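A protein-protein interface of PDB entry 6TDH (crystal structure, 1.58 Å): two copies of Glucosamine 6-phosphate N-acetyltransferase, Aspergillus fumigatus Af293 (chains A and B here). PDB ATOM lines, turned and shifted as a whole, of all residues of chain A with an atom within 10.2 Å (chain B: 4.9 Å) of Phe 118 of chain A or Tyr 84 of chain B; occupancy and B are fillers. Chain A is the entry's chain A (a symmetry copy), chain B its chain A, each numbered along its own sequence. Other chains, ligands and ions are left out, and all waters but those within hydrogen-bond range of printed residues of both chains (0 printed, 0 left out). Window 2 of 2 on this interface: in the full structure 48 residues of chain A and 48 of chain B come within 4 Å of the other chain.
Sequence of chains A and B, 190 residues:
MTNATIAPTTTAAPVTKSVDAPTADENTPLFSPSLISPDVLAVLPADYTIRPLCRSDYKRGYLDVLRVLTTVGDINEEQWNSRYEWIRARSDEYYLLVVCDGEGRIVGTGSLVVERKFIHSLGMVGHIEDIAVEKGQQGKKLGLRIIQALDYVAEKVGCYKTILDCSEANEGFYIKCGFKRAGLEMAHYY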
ATOM      1  N   VAL A 114       2.396   7.213 -34.291  1.00  0.00           N
ATOM      2  CA  VAL A 114       1.670   8.146 -33.403  1.00  0.00           C
ATOM      3  C   VAL A 114       0.376   7.441 -32.999  1.00  0.00           C
ATOM      4  O   VAL A 114      -0.438   7.142 -33.851  1.00  0.00           O
ATOM      5  CB  VAL A 114       1.470   9.514 -34.075  1.00  0.00           C
ATOM      6  CG1 VAL A 114       0.589  10.421 -33.220  1.00  0.00           C
ATOM      7  CG2 VAL A 114       2.822  10.172 -34.334  1.00  0.00           C
ATOM      8  N   GLU A 115       0.245   7.181 -31.708  1.00  0.00           N
ATOM      9  CA  GLU A 115      -0.909   6.490 -31.102  1.00  0.00           C
ATOM     10  C   GLU A 115      -1.874   7.595 -30.683  1.00  0.00           C
ATOM     11  O   GLU A 115      -1.536   8.371 -29.801  1.00  0.00           O
ATOM     12  CB  GLU A 115      -0.406   5.649 -29.928  1.00  0.00           C
ATOM     13  CG  GLU A 115      -1.467   4.757 -29.301  1.00  0.00           C
ATOM     14  CD  GLU A 115      -1.076   4.180 -27.945  1.00  0.00           C
ATOM     15  OE1 GLU A 115       0.004   4.607 -27.363  1.00  0.00           O
ATOM     16  OE2 GLU A 115      -1.883   3.343 -27.427  1.00  0.00           O
ATOM     17  N   ARG A 116      -2.948   7.753 -31.430  1.00  0.00           N
ATOM     18  CA  ARG A 116      -4.062   8.674 -31.086  1.00  0.00           C
ATOM     19  C   ARG A 116      -5.037   7.847 -30.227  1.00  0.00           C
ATOM     20  O   ARG A 116      -5.629   6.933 -30.788  1.00  0.00           O
ATOM     21  CB  ARG A 116      -4.641   9.238 -32.395  1.00  0.00           C
ATOM     22  CG  ARG A 116      -3.648  10.056 -33.222  1.00  0.00           C
ATOM     23  CD  ARG A 116      -4.065  10.477 -34.636  1.00  0.00           C
ATOM     24  NE  ARG A 116      -2.907  10.867 -35.465  1.00  0.00           N
ATOM     25  CZ  ARG A 116      -2.426  12.113 -35.651  1.00  0.00           C
ATOM     26  NH1 ARG A 116      -3.004  13.177 -35.101  1.00  0.00           N
ATOM     27  NH2 ARG A 116      -1.334  12.300 -36.397  1.00  0.00           N
ATOM     28  N   LYS A 117      -5.085   8.114 -28.917  1.00  0.00           N
ATOM     29  CA  LYS A 117      -5.977   7.501 -27.894  1.00  0.00           C
ATOM     30  C   LYS A 117      -7.464   7.759 -28.224  1.00  0.00           C
ATOM     31  O   LYS A 117      -7.826   8.885 -28.653  1.00  0.00           O
ATOM     32  CB  LYS A 117      -5.707   8.100 -26.511  1.00  0.00           C
ATOM     33  CG  LYS A 117      -4.996   7.240 -25.470  1.00  0.00           C
ATOM     34  CD  LYS A 117      -3.723   6.538 -25.896  1.00  0.00           C
ATOM     35  CE  LYS A 117      -2.830   6.197 -24.718  1.00  0.00           C
ATOM     36  NZ  LYS A 117      -2.306   4.814 -24.790  1.00  0.00           N
ATOM     37  N   PHE A 118      -8.315   6.754 -27.995  1.00  0.00           N
ATOM     38  CA  PHE A 118      -9.797   6.852 -28.037  1.00  0.00           C
ATOM     39  C   PHE A 118     -10.279   8.099 -27.277  1.00  0.00           C
ATOM     40  O   PHE A 118     -10.963   8.802 -28.097  1.00  0.00           O
ATOM     41  CB  PHE A 118     -10.438   5.570 -27.487  1.00  0.00           C
ATOM     42  CG  PHE A 118     -11.944   5.584 -27.436  1.00  0.00           C
ATOM     43  CD1 PHE A 118     -12.688   6.090 -28.488  1.00  0.00           C
ATOM     44  CD2 PHE A 118     -12.618   5.091 -26.338  1.00  0.00           C
ATOM     45  CE1 PHE A 118     -14.073   6.101 -28.448  1.00  0.00           C
ATOM     46  CE2 PHE A 118     -14.008   5.108 -26.287  1.00  0.00           C
ATOM     47  CZ  PHE A 118     -14.735   5.610 -27.346  1.00  0.00           C
ATOM     48  N   HIS A 120      -5.754  10.396 -22.482  1.00  0.00           N
ATOM     49  CA  HIS A 120      -5.016  11.567 -21.912  1.00  0.00           C
ATOM     50  C   HIS A 120      -5.786  12.858 -22.249  1.00  0.00           C
ATOM     51  O   HIS A 120      -5.163  13.852 -22.697  1.00  0.00           O
ATOM     52  CB  HIS A 120      -3.557  11.555 -22.411  1.00  0.00           C
ATOM     53  CG  HIS A 120      -2.605  12.462 -21.694  1.00  0.00           C
ATOM     54  ND1 HIS A 120      -1.923  12.061 -20.556  1.00  0.00           N
ATOM     55  CD2 HIS A 120      -2.147  13.705 -21.991  1.00  0.00           C
ATOM     56  CE1 HIS A 120      -1.105  13.026 -20.171  1.00  0.00           C
ATOM     57  NE2 HIS A 120      -1.226  14.049 -21.037  1.00  0.00           N
ATOM     58  N   SER A 121      -7.094  12.852 -21.980  1.00  0.00           N
ATOM     59  CA  SER A 121      -8.100  13.781 -22.557  1.00  0.00           C
ATOM     60  C   SER A 121      -7.993  13.626 -24.068  1.00  0.00           C
ATOM     61  O   SER A 121      -7.851  14.649 -24.733  1.00  0.00           O
ATOM     62  CB  SER A 121      -7.903  15.228 -22.145  1.00  0.00           C
ATOM     63  OG  SER A 121      -7.349  15.330 -20.846  1.00  0.00           O
ATOM     64  N   LEU A 122      -7.990  12.372 -24.535  1.00  0.00           N
ATOM     65  CA  LEU A 122      -7.825  11.926 -25.944  1.00  0.00           C
ATOM     66  C   LEU A 122      -6.391  12.180 -26.476  1.00  0.00           C
ATOM     67  O   LEU A 122      -6.247  12.199 -27.720  1.00  0.00           O
ATOM     68  CB  LEU A 122      -8.976  12.502 -26.797  1.00  0.00           C
ATOM     69  CG  LEU A 122      -8.891  13.825 -27.596  1.00  0.00           C
ATOM     70  CD1 LEU A 122      -9.882  14.867 -27.069  1.00  0.00           C
ATOM     71  CD2 LEU A 122      -7.501  14.452 -27.762  1.00  0.00           C
ATOM     72  N   GLY A 123      -5.356  12.151 -25.604  1.00  0.00           N
ATOM     73  CA  GLY A 123      -3.946  12.567 -25.862  1.00  0.00           C
ATOM     74  C   GLY A 123      -3.162  11.674 -26.839  1.00  0.00           C
ATOM     75  O   GLY A 123      -3.778  10.730 -27.370  1.00  0.00           O
ATOM     76  N   MET A 124      -1.865  11.975 -27.117  1.00  0.00           N
ATOM     77  CA  MET A 124      -1.036  11.252 -28.136  1.00  0.00           C
ATOM     78  C   MET A 124       0.376  10.882 -27.646  1.00  0.00           C
ATOM     79  O   MET A 124       1.103  11.691 -27.035  1.00  0.00           O
ATOM     80  CB  MET A 124      -0.899  12.064 -29.419  1.00  0.00           C
ATOM     81  CG  MET A 124      -2.096  11.958 -30.299  1.00  0.00           C
ATOM     82  SD  MET A 124      -2.293  13.427 -31.357  1.00  0.00           S
ATOM     83  CE  MET A 124      -1.244  14.634 -30.553  1.00  0.00           C
ATOM     84  N   VAL A 125       0.747   9.644 -27.917  1.00  0.00           N
ATOM     85  CA  VAL A 125       2.076   9.084 -27.565  1.00  0.00           C
ATOM     86  C   VAL A 125       2.768   8.698 -28.865  1.00  0.00           C
ATOM     87  O   VAL A 125       2.175   7.986 -29.667  1.00  0.00           O
ATOM     88  CB  VAL A 125       1.913   7.855 -26.647  1.00  0.00           C
ATOM     89  CG1 VAL A 125       3.264   7.250 -26.275  1.00  0.00           C
ATOM     90  CG2 VAL A 125       1.144   8.266 -25.386  1.00  0.00           C
ATOM     91  N   THR B  28     -23.780  -2.147 -32.350  1.00  0.00           N
ATOM     92  CA  THR B  28     -22.853  -2.752 -33.343  1.00  0.00           C
ATOM     93  C   THR B  28     -21.460  -2.811 -32.726  1.00  0.00           C
ATOM     94  O   THR B  28     -20.920  -1.790 -32.341  1.00  0.00           O
ATOM     95  CB  THR B  28     -22.757  -1.935 -34.628  1.00  0.00           C
ATOM     96  OG1 THR B  28     -24.075  -1.921 -35.183  1.00  0.00           O
ATOM     97  CG2 THR B  28     -21.751  -2.526 -35.590  1.00  0.00           C
ATOM     98  N   PRO B  29     -20.894  -4.001 -32.530  1.00  0.00           N
ATOM     99  CA  PRO B  29     -19.592  -4.078 -31.869  1.00  0.00           C
ATOM    100  C   PRO B  29     -18.493  -3.422 -32.722  1.00  0.00           C
ATOM    101  O   PRO B  29     -18.551  -3.467 -33.945  1.00  0.00           O
ATOM    102  CB  PRO B  29     -19.357  -5.576 -31.672  1.00  0.00           C
ATOM    103  CG  PRO B  29     -20.354  -6.275 -32.560  1.00  0.00           C
ATOM    104  CD  PRO B  29     -21.498  -5.309 -32.787  1.00  0.00           C
ATOM    105  N   LEU B  30     -17.480  -2.876 -32.051  1.00  0.00           N
ATOM    106  CA  LEU B  30     -16.282  -2.273 -32.665  1.00  0.00           C
ATOM    107  C   LEU B  30     -15.594  -3.270 -33.606  1.00  0.00           C
ATOM    108  O   LEU B  30     -15.100  -2.840 -34.662  1.00  0.00           O
ATOM    109  CB  LEU B  30     -15.331  -1.809 -31.562  1.00  0.00           C
ATOM    110  CG  LEU B  30     -14.038  -1.177 -32.047  1.00  0.00           C
ATOM    111  CD1 LEU B  30     -14.311  -0.049 -33.012  1.00  0.00           C
ATOM    112  CD2 LEU B  30     -13.191  -0.701 -30.870  1.00  0.00           C
ATOM    113  N   LEU B  53     -15.940  -3.160 -27.403  1.00  0.00           N
ATOM    114  CA  LEU B  53     -16.619  -1.876 -27.180  1.00  0.00           C
ATOM    115  C   LEU B  53     -17.752  -1.715 -28.178  1.00  0.00           C
ATOM    116  O   LEU B  53     -17.625  -2.215 -29.282  1.00  0.00           O
ATOM    117  CB  LEU B  53     -15.603  -0.761 -27.374  1.00  0.00           C
ATOM    118  CG  LEU B  53     -16.152   0.634 -27.101  1.00  0.00           C
ATOM    119  CD1 LEU B  53     -16.407   0.801 -25.598  1.00  0.00           C
ATOM    120  CD2 LEU B  53     -15.091   1.641 -27.575  1.00  0.00           C
ATOM    121  N   CYS B  54     -18.852  -1.118 -27.755  1.00  0.00           N
ATOM    122  CA  CYS B  54     -19.834  -0.615 -28.743  1.00  0.00           C
ATOM    123  C   CYS B  54     -20.221   0.805 -28.365  1.00  0.00           C
ATOM    124  O   CYS B  54     -19.874   1.293 -27.269  1.00  0.00           O
ATOM    125  CB  CYS B  54     -20.999  -1.560 -28.957  1.00  0.00           C
ATOM    126  SG  CYS B  54     -22.012  -1.672 -27.479  1.00  0.00           S
ATOM    127  N   ARG B  55     -20.880   1.470 -29.296  1.00  0.00           N
ATOM    128  CA  ARG B  55     -21.062   2.934 -29.182  1.00  0.00           C
ATOM    129  C   ARG B  55     -21.937   3.215 -27.955  1.00  0.00           C
ATOM    130  O   ARG B  55     -21.679   4.234 -27.247  1.00  0.00           O
ATOM    131  CB  ARG B  55     -21.633   3.528 -30.473  1.00  0.00           C
ATOM    132  CG  ARG B  55     -21.391   5.024 -30.602  1.00  0.00           C
ATOM    133  CD  ARG B  55     -21.853   5.612 -31.928  1.00  0.00           C
ATOM    134  NE  ARG B  55     -23.261   5.355 -32.223  1.00  0.00           N
ATOM    135  CZ  ARG B  55     -23.746   4.346 -32.958  1.00  0.00           C
ATOM    136  NH1 ARG B  55     -22.949   3.437 -33.511  1.00  0.00           N
ATOM    137  NH2 ARG B  55     -25.056   4.255 -33.142  1.00  0.00           N
ATOM    138  N   TYR B  62     -18.200   3.421 -19.153  1.00  0.00           N
ATOM    139  CA  TYR B  62     -16.840   3.221 -19.699  1.00  0.00           C
ATOM    140  C   TYR B  62     -15.870   4.310 -19.192  1.00  0.00           C
ATOM    141  O   TYR B  62     -14.836   3.930 -18.687  1.00  0.00           O
ATOM    142  CB  TYR B  62     -16.872   3.198 -21.220  1.00  0.00           C
ATOM    143  CG  TYR B  62     -15.509   3.059 -21.826  1.00  0.00           C
ATOM    144  CD1 TYR B  62     -14.936   1.803 -21.968  1.00  0.00           C
ATOM    145  CD2 TYR B  62     -14.774   4.163 -22.235  1.00  0.00           C
ATOM    146  CE1 TYR B  62     -13.685   1.634 -22.517  1.00  0.00           C
ATOM    147  CE2 TYR B  62     -13.511   4.005 -22.782  1.00  0.00           C
ATOM    148  CZ  TYR B  62     -12.969   2.738 -22.929  1.00  0.00           C
ATOM    149  OH  TYR B  62     -11.750   2.534 -23.505  1.00  0.00           O
ATOM    150  N   GLN B  79     -19.376  14.077 -28.533  1.00  0.00           N
ATOM    151  CA  GLN B  79     -17.897  13.929 -28.590  1.00  0.00           C
ATOM    152  C   GLN B  79     -17.566  12.430 -28.618  1.00  0.00           C
ATOM    153  O   GLN B  79     -16.667  12.001 -29.383  1.00  0.00           O
ATOM    154  CB  GLN B  79     -17.228  14.507 -27.349  1.00  0.00           C
ATOM    155  CG  GLN B  79     -17.135  16.023 -27.304  1.00  0.00           C
ATOM    156  CD  GLN B  79     -15.786  16.411 -26.747  1.00  0.00           C
ATOM    157  OE1 GLN B  79     -15.651  16.764 -25.575  1.00  0.00           O
ATOM    158  NE2 GLN B  79     -14.768  16.270 -27.583  1.00  0.00           N
ATOM    159  N   TRP B  80     -18.210  11.701 -27.710  1.00  0.00           N
ATOM    160  CA  TRP B  80     -18.138  10.214 -27.642  1.00  0.00           C
ATOM    161  C   TRP B  80     -18.431   9.639 -29.028  1.00  0.00           C
ATOM    162  O   TRP B  80     -17.614   8.855 -29.539  1.00  0.00           O
ATOM    163  CB  TRP B  80     -19.142   9.669 -26.615  1.00  0.00           C
ATOM    164  CG  TRP B  80     -19.243   8.172 -26.686  1.00  0.00           C
ATOM    165  CD1 TRP B  80     -20.068   7.439 -27.474  1.00  0.00           C
ATOM    166  CD2 TRP B  80     -18.417   7.235 -25.984  1.00  0.00           C
ATOM    167  NE1 TRP B  80     -19.819   6.094 -27.317  1.00  0.00           N
ATOM    168  CE2 TRP B  80     -18.820   5.943 -26.396  1.00  0.00           C
ATOM    169  CE3 TRP B  80     -17.392   7.355 -25.039  1.00  0.00           C
ATOM    170  CZ2 TRP B  80     -18.259   4.784 -25.852  1.00  0.00           C
ATOM    171  CZ3 TRP B  80     -16.823   6.209 -24.519  1.00  0.00           C
ATOM    172  CH2 TRP B  80     -17.236   4.942 -24.954  1.00  0.00           C
ATOM    173  N   ASN B  81     -19.571  10.015 -29.612  1.00  0.00           N
ATOM    174  CA  ASN B  81     -20.013   9.533 -30.945  1.00  0.00           C
ATOM    175  C   ASN B  81     -18.931   9.814 -31.991  1.00  0.00           C
ATOM    176  O   ASN B  81     -18.653   8.917 -32.800  1.00  0.00           O
ATOM    177  CB  ASN B  81     -21.370  10.123 -31.321  1.00  0.00           C
ATOM    178  CG  ASN B  81     -22.463   9.420 -30.558  1.00  0.00           C
ATOM    179  OD1 ASN B  81     -22.183   8.436 -29.875  1.00  0.00           O
ATOM    180  ND2 ASN B  81     -23.680   9.937 -30.635  1.00  0.00           N
ATOM    181  N   SER B  82     -18.314  10.999 -31.975  1.00  0.00           N
ATOM    182  CA  SER B  82     -17.245  11.338 -32.953  1.00  0.00           C
ATOM    183  C   SER B  82     -15.991  10.520 -32.668  1.00  0.00           C
ATOM    184  O   SER B  82     -15.358  10.073 -33.638  1.00  0.00           O
ATOM    185  CB  SER B  82     -16.924  12.832 -33.003  1.00  0.00           C
ATOM    186  OG  SER B  82     -18.130  13.545 -33.192  1.00  0.00           O
ATOM    187  N   ARG B  83     -15.628  10.340 -31.406  1.00  0.00           N
ATOM    188  CA  ARG B  83     -14.394   9.576 -31.062  1.00  0.00           C
ATOM    189  C   ARG B  83     -14.627   8.104 -31.416  1.00  0.00           C
ATOM    190  O   ARG B  83     -13.709   7.472 -31.984  1.00  0.00           O
ATOM    191  CB  ARG B  83     -13.966   9.779 -29.604  1.00  0.00           C
ATOM    192  CG  ARG B  83     -12.966  10.924 -29.450  1.00  0.00           C
ATOM    193  CD  ARG B  83     -11.812  10.668 -30.411  1.00  0.00           C
ATOM    194  NE  ARG B  83     -10.697  11.594 -30.329  1.00  0.00           N
ATOM    195  CZ  ARG B  83     -10.725  12.839 -30.794  1.00  0.00           C
ATOM    196  NH1 ARG B  83     -11.833  13.323 -31.337  1.00  0.00           N
ATOM    197  NH2 ARG B  83      -9.655  13.612 -30.694  1.00  0.00           N
ATOM    198  N   TYR B  84     -15.849   7.620 -31.208  1.00  0.00           N
ATOM    199  CA  TYR B  84     -16.227   6.231 -31.587  1.00  0.00           C
ATOM    200  C   TYR B  84     -16.118   6.016 -33.118  1.00  0.00           C
ATOM    201  O   TYR B  84     -15.577   4.959 -33.550  1.00  0.00           O
ATOM    202  CB  TYR B  84     -17.626   5.874 -31.092  1.00  0.00           C
ATOM    203  CG  TYR B  84     -17.878   4.400 -31.268  1.00  0.00           C
ATOM    204  CD1 TYR B  84     -17.361   3.497 -30.358  1.00  0.00           C
ATOM    205  CD2 TYR B  84     -18.476   3.905 -32.408  1.00  0.00           C
ATOM    206  CE1 TYR B  84     -17.524   2.129 -30.552  1.00  0.00           C
ATOM    207  CE2 TYR B  84     -18.641   2.541 -32.606  1.00  0.00           C
ATOM    208  CZ  TYR B  84     -18.193   1.656 -31.644  1.00  0.00           C
ATOM    209  OH  TYR B  84     -18.295   0.303 -31.805  1.00  0.00           O
ATOM    210  N   GLU B  85     -16.632   6.930 -33.951  1.00  0.00           N
ATOM    211  CA  GLU B  85     -16.502   6.810 -35.433  1.00  0.00           C
ATOM    212  C   GLU B  85     -15.019   6.846 -35.829  1.00  0.00           C
ATOM    213  O   GLU B  85     -14.627   6.081 -36.719  1.00  0.00           O
ATOM    214  CB  GLU B  85     -17.359   7.853 -36.147  1.00  0.00           C
ATOM    215  CG  GLU B  85     -18.863   7.622 -35.952  1.00  0.00           C
ATOM    216  CD  GLU B  85     -19.387   6.207 -36.205  1.00  0.00           C
ATOM    217  OE1 GLU B  85     -20.093   5.655 -35.330  1.00  0.00           O
ATOM    218  OE2 GLU B  85     -19.095   5.655 -37.287  1.00  0.00           O
ATOM    219  N   TRP B  86     -14.211   7.672 -35.171  1.00  0.00           N
ATOM    220  CA  TRP B  86     -12.755   7.763 -35.409  1.00  0.00           C
ATOM    221  C   TRP B  86     -12.083   6.397 -35.170  1.00  0.00           C
ATOM    222  O   TRP B  86     -11.368   5.927 -36.056  1.00  0.00           O
ATOM    223  CB  TRP B  86     -12.120   8.887 -34.573  1.00  0.00           C
ATOM    224  CG  TRP B  86     -10.689   9.060 -34.960  1.00  0.00           C
ATOM    225  CD1 TRP B  86     -10.198   9.716 -36.052  1.00  0.00           C
ATOM    226  CD2 TRP B  86      -9.572   8.401 -34.344  1.00  0.00           C
ATOM    227  NE1 TRP B  86      -8.839   9.569 -36.114  1.00  0.00           N
ATOM    228  CE2 TRP B  86      -8.432   8.743 -35.097  1.00  0.00           C
ATOM    229  CE3 TRP B  86      -9.432   7.564 -33.230  1.00  0.00           C
ATOM    230  CZ2 TRP B  86      -7.160   8.299 -34.746  1.00  0.00           C
ATOM    231  CZ3 TRP B  86      -8.177   7.106 -32.902  1.00  0.00           C
ATOM    232  CH2 TRP B  86      -7.062   7.469 -33.650  1.00  0.00           C
ATOM    233  N   ILE B  87     -12.337   5.737 -34.041  1.00  0.00           N
ATOM    234  CA  ILE B  87     -11.673   4.430 -33.736  1.00  0.00           C
ATOM    235  C   ILE B  87     -12.208   3.363 -34.693  1.00  0.00           C
ATOM    236  O   ILE B  87     -11.407   2.519 -35.145  1.00  0.00           O
ATOM    237  CB  ILE B  87     -11.873   4.018 -32.260  1.00  0.00           C
ATOM    238  CG1 ILE B  87     -11.080   4.915 -31.313  1.00  0.00           C
ATOM    239  CG2 ILE B  87     -11.507   2.557 -32.041  1.00  0.00           C
ATOM    240  CD1 ILE B  87      -9.591   4.663 -31.328  1.00  0.00           C
ATOM    241  N   ARG B  88     -13.507   3.375 -34.965  1.00  0.00           N
ATOM    242  CA  ARG B  88     -14.187   2.415 -35.874  1.00  0.00           C
ATOM    243  C   ARG B  88     -13.549   2.531 -37.265  1.00  0.00           C
ATOM    244  O   ARG B  88     -13.387   1.511 -37.880  1.00  0.00           O
ATOM    245  CB  ARG B  88     -15.699   2.645 -35.953  1.00  0.00           C
ATOM    246  CG  ARG B  88     -16.479   1.500 -36.585  1.00  0.00           C
ATOM    247  CD  ARG B  88     -17.853   1.917 -37.100  1.00  0.00           C
ATOM    248  NE  ARG B  88     -17.870   3.296 -37.591  1.00  0.00           N
ATOM    249  CZ  ARG B  88     -17.287   3.735 -38.716  1.00  0.00           C
ATOM    250  NH1 ARG B  88     -16.636   2.906 -39.517  1.00  0.00           N
ATOM    251  NH2 ARG B  88     -17.350   5.018 -39.034  1.00  0.00           N
ATOM    252  N   LEU B  96     -10.466  -2.447 -28.770  1.00  0.00           N
ATOM    253  CA  LEU B  96     -10.867  -2.042 -27.411  1.00  0.00           C
ATOM    254  C   LEU B  96     -11.960  -2.987 -26.927  1.00  0.00           C
ATOM    255  O   LEU B  96     -13.011  -3.134 -27.595  1.00  0.00           O
ATOM    256  CB  LEU B  96     -11.358  -0.605 -27.389  1.00  0.00           C
ATOM    257  CG  LEU B  96     -10.287   0.445 -27.259  1.00  0.00           C
ATOM    258  CD1 LEU B  96      -9.333   0.374 -28.439  1.00  0.00           C
ATOM    259  CD2 LEU B  96     -10.935   1.827 -27.075  1.00  0.00           C
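No position is printed for both chains. Of the 9 pairs that touch across the chains among the printed residues, none has its exchanged pair printed and touching as well.
O of Arg 116 of chain A touches CH2 of Trp 86 of chain B, 3.2 Å away. CE2 of Phe 118 of chain A touches CD2 of Leu 53 of chain B, at 3.9 Å. CE2 of Phe 118 of chain A touches CE2 of Tyr 62 of chain B, 3.7 Å away. Trp 80 of chain B touches Phe 118 of chain A. Phe 118 of chain A touches Arg 83 of chain B (O to CD, 3.1 Å). Phe 118 of chain A touches Tyr 84 of chain B. Ile 87 of chain B touches Phe 118 of chain A. Phe 118 of chain A touches Leu 96 of chain B. Leu 122 of chain A touches Arg 83 of chain B.
The side-chain hydroxyl (OH) of Tyr 84 of chain B sits at hydrogen-bond distance from the backbone carbonyl oxygen (O) of Thr 28 of chain B, 3.4 Å away. The backbone NH (N) of Leu 30 of chain B is in hydrogen-bond range of the backbone carbonyl oxygen (O) of Leu 53 of chain B (2.9 Å). The backbone NH of Leu 30 of chain B sits at hydrogen-bond distance from the side-chain hydroxyl of Tyr 84 of chain B (3.3 Å). The backbone NH of Leu 53 of chain B sits at hydrogen-bond distance from the backbone carbonyl oxygen of Leu 96 of chain B. The backbone carbonyl oxygen of Arg 55 of chain B lies within hydrogen-bond range of the indole nitrogen of Trp 80 of chain B, 2.6 Å away.
Of the printed residues of chain B, Arg 116 of chain A touches Trp 86. Of chain B, only Leu 53, Tyr 62, Trp 80, Arg 83, Tyr 84, Ile 87 and Leu 96 come within 4 Å of Phe 118 of chain A. Thr 28 of chain B touches none of the printed residues of chain A. No residue of chain A comes within 4 Å of Leu 30 of chain B. Leu 53 of chain B touches one residue of chain A. No residue of chain A comes within 4 Å of Cys 54 of chain B. Of the printed residues of chain A, Tyr 62 of chain B touches Phe 118. Of chain A, only Phe 118 (3.5 Å) comes within 4 Å of Trp 80 of chain B. Of chain A, only Phe 118 and Leu 122 come within 4 Å of Arg 83 of chain B. Tyr 84 of chain B touches just one residue of chain A: Phe 118. No residue of chain A comes within 4 Å of Glu 85 of chain B. Arg 88 of chain B touches none of the printed residues of chain A. The nearest printed residue of chain B that does not touch Phe 118 of chain A is Trp 86 of chain B (4.9 Å). The nearest printed residue of chain A that does not touch Trp 86 of chain B is Lys 117 of chain A (4.6 Å).
Printed residues of chain A that touch a printed residue of chain B: Arg 116, Phe 118 and Leu 122. Hydrophobic or aromatic side chains of chain A within 4 Å of the printed part of chain B: Phe 118 and Leu 122. Along chain A the printed residues that touch a printed residue of chain B span positions 116 to 122. Of the 18 printed residues of chain B, 8 touch a printed residue of chain A. Printed residues of chain B that touch a printed residue of chain A: Leu 53, Tyr 62, Trp 80, Arg 83, Tyr 84, Trp 86, Ile 87 and Leu 96. Among the printed residues, no Asp or Glu carboxylate lies within 4 Å of a Lys or Arg side-chain nitrogen of the other chain.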
